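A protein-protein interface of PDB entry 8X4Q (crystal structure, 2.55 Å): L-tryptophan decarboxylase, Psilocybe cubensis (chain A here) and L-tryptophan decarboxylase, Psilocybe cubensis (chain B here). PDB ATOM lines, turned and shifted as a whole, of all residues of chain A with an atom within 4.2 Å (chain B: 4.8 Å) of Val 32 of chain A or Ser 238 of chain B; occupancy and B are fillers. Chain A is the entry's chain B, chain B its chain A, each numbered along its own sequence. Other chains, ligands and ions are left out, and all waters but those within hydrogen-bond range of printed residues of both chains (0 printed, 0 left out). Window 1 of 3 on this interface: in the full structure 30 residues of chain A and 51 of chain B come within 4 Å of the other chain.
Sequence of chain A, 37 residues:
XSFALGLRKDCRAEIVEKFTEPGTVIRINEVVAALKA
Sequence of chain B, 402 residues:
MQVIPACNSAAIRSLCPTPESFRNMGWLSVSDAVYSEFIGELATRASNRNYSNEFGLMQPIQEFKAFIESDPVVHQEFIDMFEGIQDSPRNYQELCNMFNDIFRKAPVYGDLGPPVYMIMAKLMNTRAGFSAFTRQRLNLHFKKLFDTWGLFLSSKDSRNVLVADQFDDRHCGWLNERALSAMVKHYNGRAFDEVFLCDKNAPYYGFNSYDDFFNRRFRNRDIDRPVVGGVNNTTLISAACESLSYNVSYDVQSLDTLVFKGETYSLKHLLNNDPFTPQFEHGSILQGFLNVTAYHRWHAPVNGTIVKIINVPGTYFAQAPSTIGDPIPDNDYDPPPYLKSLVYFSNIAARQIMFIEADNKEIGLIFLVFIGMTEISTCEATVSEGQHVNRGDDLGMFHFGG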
ATOM      1  N   LEU A   5     -13.405  25.704  22.360  1.00  0.00           N
ATOM      2  CA  LEU A   5     -12.668  24.492  22.034  1.00  0.00           C
ATOM      3  C   LEU A   5     -12.919  23.469  23.139  1.00  0.00           C
ATOM      4  O   LEU A   5     -12.844  23.810  24.327  1.00  0.00           O
ATOM      5  CB  LEU A   5     -11.179  24.795  21.902  1.00  0.00           C
ATOM      6  CG  LEU A   5     -10.267  23.586  21.752  1.00  0.00           C
ATOM      7  CD1 LEU A   5     -10.282  23.119  20.302  1.00  0.00           C
ATOM      8  CD2 LEU A   5      -8.861  23.944  22.189  1.00  0.00           C
ATOM      9  N   ILE A  15      -4.520  22.651  28.324  1.00  0.00           N
ATOM     10  CA  ILE A  15      -4.704  24.061  28.008  1.00  0.00           C
ATOM     11  C   ILE A  15      -3.556  24.870  28.599  1.00  0.00           C
ATOM     12  O   ILE A  15      -3.121  24.640  29.732  1.00  0.00           O
ATOM     13  CB  ILE A  15      -6.071  24.548  28.517  1.00  0.00           C
ATOM     14  CG1 ILE A  15      -7.175  23.829  27.769  1.00  0.00           C
ATOM     15  CG2 ILE A  15      -6.225  26.057  28.342  1.00  0.00           C
ATOM     16  CD1 ILE A  15      -8.523  24.002  28.395  1.00  0.00           C
ATOM     17  N   VAL A  16      -3.030  25.805  27.809  1.00  0.00           N
ATOM     18  CA  VAL A  16      -1.958  26.661  28.285  1.00  0.00           C
ATOM     19  C   VAL A  16      -2.480  27.499  29.440  1.00  0.00           C
ATOM     20  O   VAL A  16      -3.562  28.099  29.357  1.00  0.00           O
ATOM     21  CB  VAL A  16      -1.424  27.516  27.130  1.00  0.00           C
ATOM     22  CG1 VAL A  16      -0.403  28.521  27.631  1.00  0.00           C
ATOM     23  CG2 VAL A  16      -0.862  26.610  26.052  1.00  0.00           C
ATOM     24  N   PHE A  19      -4.227  31.148  29.766  1.00  0.00           N
ATOM     25  CA  PHE A  19      -5.555  31.462  29.259  1.00  0.00           C
ATOM     26  C   PHE A  19      -6.646  31.207  30.278  1.00  0.00           C
ATOM     27  O   PHE A  19      -7.805  31.535  30.009  1.00  0.00           O
ATOM     28  CB  PHE A  19      -5.833  30.693  27.972  1.00  0.00           C
ATOM     29  CG  PHE A  19      -4.900  31.054  26.867  1.00  0.00           C
ATOM     30  CD1 PHE A  19      -4.779  32.382  26.461  1.00  0.00           C
ATOM     31  CD2 PHE A  19      -4.113  30.091  26.252  1.00  0.00           C
ATOM     32  CE1 PHE A  19      -3.908  32.742  25.442  1.00  0.00           C
ATOM     33  CE2 PHE A  19      -3.242  30.445  25.225  1.00  0.00           C
ATOM     34  CZ  PHE A  19      -3.139  31.771  24.821  1.00  0.00           C
ATOM     35  N   ASN A  29      -4.214  31.429  15.785  1.00  0.00           N
ATOM     36  CA  ASN A  29      -3.166  30.472  15.446  1.00  0.00           C
ATOM     37  C   ASN A  29      -2.147  30.247  16.569  1.00  0.00           C
ATOM     38  O   ASN A  29      -1.355  29.314  16.461  1.00  0.00           O
ATOM     39  CB  ASN A  29      -2.386  30.844  14.169  1.00  0.00           C
ATOM     40  CG  ASN A  29      -3.244  30.823  12.946  1.00  0.00           C
ATOM     41  OD1 ASN A  29      -4.161  30.024  12.856  1.00  0.00           O
ATOM     42  ND2 ASN A  29      -2.954  31.703  11.987  1.00  0.00           N
ATOM     43  N   GLU A  30      -2.104  31.062  17.624  1.00  0.00           N
ATOM     44  CA  GLU A  30      -1.127  30.746  18.661  1.00  0.00           C
ATOM     45  C   GLU A  30      -1.587  29.513  19.437  1.00  0.00           C
ATOM     46  O   GLU A  30      -2.718  29.036  19.284  1.00  0.00           O
ATOM     47  CB  GLU A  30      -0.884  31.938  19.592  1.00  0.00           C
ATOM     48  CG  GLU A  30      -1.831  32.055  20.789  1.00  0.00           C
ATOM     49  CD  GLU A  30      -1.408  33.169  21.752  1.00  0.00           C
ATOM     50  OE1 GLU A  30      -0.451  32.954  22.539  1.00  0.00           O
ATOM     51  OE2 GLU A  30      -2.027  34.261  21.715  1.00  0.00           O
ATOM     52  N   VAL A  31      -0.684  28.981  20.256  1.00  0.00           N
ATOM     53  CA  VAL A  31      -0.905  27.703  20.919  1.00  0.00           C
ATOM     54  C   VAL A  31      -1.798  27.924  22.141  1.00  0.00           C
ATOM     55  O   VAL A  31      -1.460  28.705  23.038  1.00  0.00           O
ATOM     56  CB  VAL A  31       0.432  27.044  21.304  1.00  0.00           C
ATOM     57  CG1 VAL A  31       0.215  25.732  22.050  1.00  0.00           C
ATOM     58  CG2 VAL A  31       1.253  26.787  20.074  1.00  0.00           C
ATOM     59  N   VAL A  32      -2.946  27.243  22.169  1.00  0.00           N
ATOM     60  CA  VAL A  32      -3.835  27.286  23.323  1.00  0.00           C
ATOM     61  C   VAL A  32      -3.879  25.966  24.084  1.00  0.00           C
ATOM     62  O   VAL A  32      -4.447  25.923  25.189  1.00  0.00           O
ATOM     63  CB  VAL A  32      -5.263  27.725  22.925  1.00  0.00           C
ATOM     64  CG1 VAL A  32      -5.236  29.171  22.394  1.00  0.00           C
ATOM     65  CG2 VAL A  32      -5.892  26.734  21.929  1.00  0.00           C
ATOM     66  N   ALA A  33      -3.308  24.896  23.539  1.00  0.00           N
ATOM     67  CA  ALA A  33      -3.175  23.627  24.239  1.00  0.00           C
ATOM     68  C   ALA A  33      -2.081  22.825  23.546  1.00  0.00           C
ATOM     69  O   ALA A  33      -1.886  22.940  22.332  1.00  0.00           O
ATOM     70  CB  ALA A  33      -4.486  22.834  24.259  1.00  0.00           C
ATOM     71  N   VAL B 227       1.351  30.240  12.532  1.00  0.00           N
ATOM     72  CA  VAL B 227       0.966  28.951  13.089  1.00  0.00           C
ATOM     73  C   VAL B 227       2.127  28.491  13.967  1.00  0.00           C
ATOM     74  O   VAL B 227       3.076  27.868  13.469  1.00  0.00           O
ATOM     75  CB  VAL B 227       0.647  27.933  11.972  1.00  0.00           C
ATOM     76  CG1 VAL B 227       0.359  26.565  12.542  1.00  0.00           C
ATOM     77  CG2 VAL B 227      -0.524  28.399  11.116  1.00  0.00           C
ATOM     78  N   LEU B 236       0.455  20.471  18.878  1.00  0.00           N
ATOM     79  CA  LEU B 236       0.038  21.801  19.291  1.00  0.00           C
ATOM     80  C   LEU B 236      -1.350  22.086  18.722  1.00  0.00           C
ATOM     81  O   LEU B 236      -1.624  21.788  17.551  1.00  0.00           O
ATOM     82  CB  LEU B 236       1.061  22.849  18.817  1.00  0.00           C
ATOM     83  CG  LEU B 236       2.525  22.613  19.233  1.00  0.00           C
ATOM     84  CD1 LEU B 236       3.446  23.716  18.786  1.00  0.00           C
ATOM     85  CD2 LEU B 236       2.649  22.460  20.719  1.00  0.00           C
ATOM     86  N   ILE B 237      -2.234  22.629  19.556  1.00  0.00           N
ATOM     87  CA  ILE B 237      -3.583  23.007  19.144  1.00  0.00           C
ATOM     88  C   ILE B 237      -3.661  24.527  19.108  1.00  0.00           C
ATOM     89  O   ILE B 237      -3.489  25.186  20.145  1.00  0.00           O
ATOM     90  CB  ILE B 237      -4.650  22.423  20.079  1.00  0.00           C
ATOM     91  CG1 ILE B 237      -4.489  20.903  20.193  1.00  0.00           C
ATOM     92  CG2 ILE B 237      -6.041  22.824  19.609  1.00  0.00           C
ATOM     93  CD1 ILE B 237      -5.353  20.289  21.268  1.00  0.00           C
ATOM     94  N   SER B 238      -3.898  25.082  17.912  1.00  0.00           N
ATOM     95  CA  SER B 238      -3.977  26.520  17.697  1.00  0.00           C
ATOM     96  C   SER B 238      -5.326  27.083  18.124  1.00  0.00           C
ATOM     97  O   SER B 238      -6.341  26.384  18.170  1.00  0.00           O
ATOM     98  CB  SER B 238      -3.766  26.874  16.224  1.00  0.00           C
ATOM     99  OG  SER B 238      -2.395  27.005  15.919  1.00  0.00           O
ATOM    100  N   ALA B 239      -5.327  28.383  18.409  1.00  0.00           N
ATOM    101  CA  ALA B 239      -6.575  29.108  18.606  1.00  0.00           C
ATOM    102  C   ALA B 239      -7.307  29.258  17.285  1.00  0.00           C
ATOM    103  O   ALA B 239      -6.734  29.739  16.300  1.00  0.00           O
ATOM    104  CB  ALA B 239      -6.311  30.489  19.194  1.00  0.00           C
ATOM    105  N   ALA B 240      -8.583  28.878  17.274  1.00  0.00           N
ATOM    106  CA  ALA B 240      -9.403  29.017  16.077  1.00  0.00           C
ATOM    107  C   ALA B 240      -9.867  30.452  15.817  1.00  0.00           C
ATOM    108  O   ALA B 240     -10.296  30.749  14.694  1.00  0.00           O
ATOM    109  CB  ALA B 240     -10.611  28.087  16.178  1.00  0.00           C
ATOM    110  N   LEU B 286     -12.213  25.595  26.649  1.00  0.00           N
ATOM    111  CA  LEU B 286     -11.686  26.961  26.626  1.00  0.00           C
ATOM    112  C   LEU B 286     -12.573  27.820  25.738  1.00  0.00           C
ATOM    113  O   LEU B 286     -12.843  27.452  24.592  1.00  0.00           O
ATOM    114  CB  LEU B 286     -10.240  27.007  26.126  1.00  0.00           C
ATOM    115  CG  LEU B 286      -9.690  28.314  25.527  1.00  0.00           C
ATOM    116  CD1 LEU B 286      -9.759  29.492  26.483  1.00  0.00           C
ATOM    117  CD2 LEU B 286      -8.257  28.129  25.049  1.00  0.00           C
ATOM    118  N   ALA B 300      -8.324  26.619  11.412  1.00  0.00           N
ATOM    119  CA  ALA B 300      -8.405  25.228  11.868  1.00  0.00           C
ATOM    120  C   ALA B 300      -7.507  25.002  13.081  1.00  0.00           C
ATOM    121  O   ALA B 300      -6.305  25.301  13.032  1.00  0.00           O
ATOM    122  CB  ALA B 300      -8.025  24.263  10.755  1.00  0.00           C
ATOM    123  N   PRO B 301      -8.042  24.475  14.175  1.00  0.00           N
ATOM    124  CA  PRO B 301      -7.239  24.358  15.399  1.00  0.00           C
ATOM    125  C   PRO B 301      -6.206  23.242  15.358  1.00  0.00           C
ATOM    126  O   PRO B 301      -5.329  23.204  16.230  1.00  0.00           O
ATOM    127  CB  PRO B 301      -8.304  24.100  16.478  1.00  0.00           C
ATOM    128  CG  PRO B 301      -9.407  23.405  15.729  1.00  0.00           C
ATOM    129  CD  PRO B 301      -9.443  24.063  14.379  1.00  0.00           C
ATOM    130  N   ARG B 391      -3.765  22.671  10.348  1.00  0.00           N
ATOM    131  CA  ARG B 391      -3.855  23.667  11.413  1.00  0.00           C
ATOM    132  C   ARG B 391      -3.562  25.061  10.876  1.00  0.00           C
ATOM    133  O   ARG B 391      -2.517  25.300  10.270  1.00  0.00           O
ATOM    134  CB  ARG B 391      -2.889  23.304  12.548  1.00  0.00           C
ATOM    135  CG  ARG B 391      -3.055  24.148  13.795  1.00  0.00           C
ATOM    136  CD  ARG B 391      -2.203  23.659  14.964  1.00  0.00           C
ATOM    137  NE  ARG B 391      -0.786  23.672  14.641  1.00  0.00           N
ATOM    138  CZ  ARG B 391       0.117  24.436  15.243  1.00  0.00           C
ATOM    139  NH1 ARG B 391      -0.227  25.301  16.187  1.00  0.00           N
ATOM    140  NH2 ARG B 391       1.395  24.341  14.877  1.00  0.00           N
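The backbone NH of Ala 239 of chain B lies within hydrogen-bond range of the backbone carbonyl oxygen of Glu 30 of chain A. The backbone carbonyl oxygen (O) of Ala 239 of chain B lies within hydrogen-bond range of the backbone NH (N) of Asn 29 of chain A (3.1 Å). The backbone carbonyl oxygen of Ile 237 of chain B sits at hydrogen-bond distance from the backbone NH of Val 32 of chain A, at 2.9 Å. O of Asn 29 of chain A is in hydrogen-bond range of OG of Ser 238 of chain B (2.6 Å). O of Leu 286 of chain B lies within hydrogen-bond range of N of Leu 5 of chain A (2.9 Å). The backbone NH (N) of Ile 237 of chain B sits at hydrogen-bond distance from the backbone carbonyl oxygen (O) of Ala 33 of chain A (2.8 Å).
N of Ser 238 of chain B lies within hydrogen-bond range of O of Pro 301 of chain B. The backbone NH (N) of Val 16 of chain A is in hydrogen-bond range of the backbone carbonyl oxygen (O) of Val 32 of chain A (3.0 Å). OG of Ser 238 of chain B is in hydrogen-bond range of NH1 of Arg 391 of chain B, 2.8 Å away.
CG2 of Ile 237 of chain B touches CD2 of Leu 5 of chain A (3.98 Å). CA of Val 227 of chain B touches CB of Asn 29 of chain A, at 3.998 Å. Glu 30 of chain A touches Ser 238 of chain B (O to CA, 3.2 Å). Val 31 of chain A touches Leu 236 of chain B. Val 31 of chain A touches Ile 237 of chain B (CA to O, 3.7 Å). CG2 of Val 32 of chain A touches O of Ser 238 of chain B, 3.8 Å away. Val 32 of chain A touches Ala 239 of chain B. Val 32 of chain A touches Leu 286 of chain B (CB to CD2, 3.7 Å). Ala 33 of chain A touches Leu 236 of chain B.
Val 32 of chain A touches four residues of chain B. Of chain A, only Asn 29 (2.6 Å), Glu 30 (3.2 Å) and Val 32 (3.8 Å) come within 4 Å of Ser 238 of chain B. Of the printed residues of chain B, Leu 5 of chain A touches Ile 237 (3.98 Å) and Leu 286 (2.9 Å). Of the printed residues of chain A, Val 227 of chain B touches Asn 29 (3.998 Å). Of the printed residues of chain A, Ile 237 of chain B touches Leu 5, Val 31, Val 32 and Ala 33. Pro 301 of chain B touches none of the printed residues of chain A. The nearest printed residue of chain B that does not touch Val 32 of chain A is Ala 240 of chain B (5.8 Å). The nearest printed residue of chain A that does not touch Ile 237 of chain B is Glu 30 of chain A (4.02 Å).
Of the 9 printed residues of chain A, 6 touch a printed residue of chain B. Printed residues of chain A that touch a printed residue of chain B: Leu 5, Asn 29, Glu 30, Val 31, Val 32 and Ala 33. Hydrophobic or aromatic side chains of chain A that line the printed part of chain B: Leu 5, Val 31 and Val 32. Along chain A the printed residues that touch a printed residue of chain B span positions 5 to 33.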
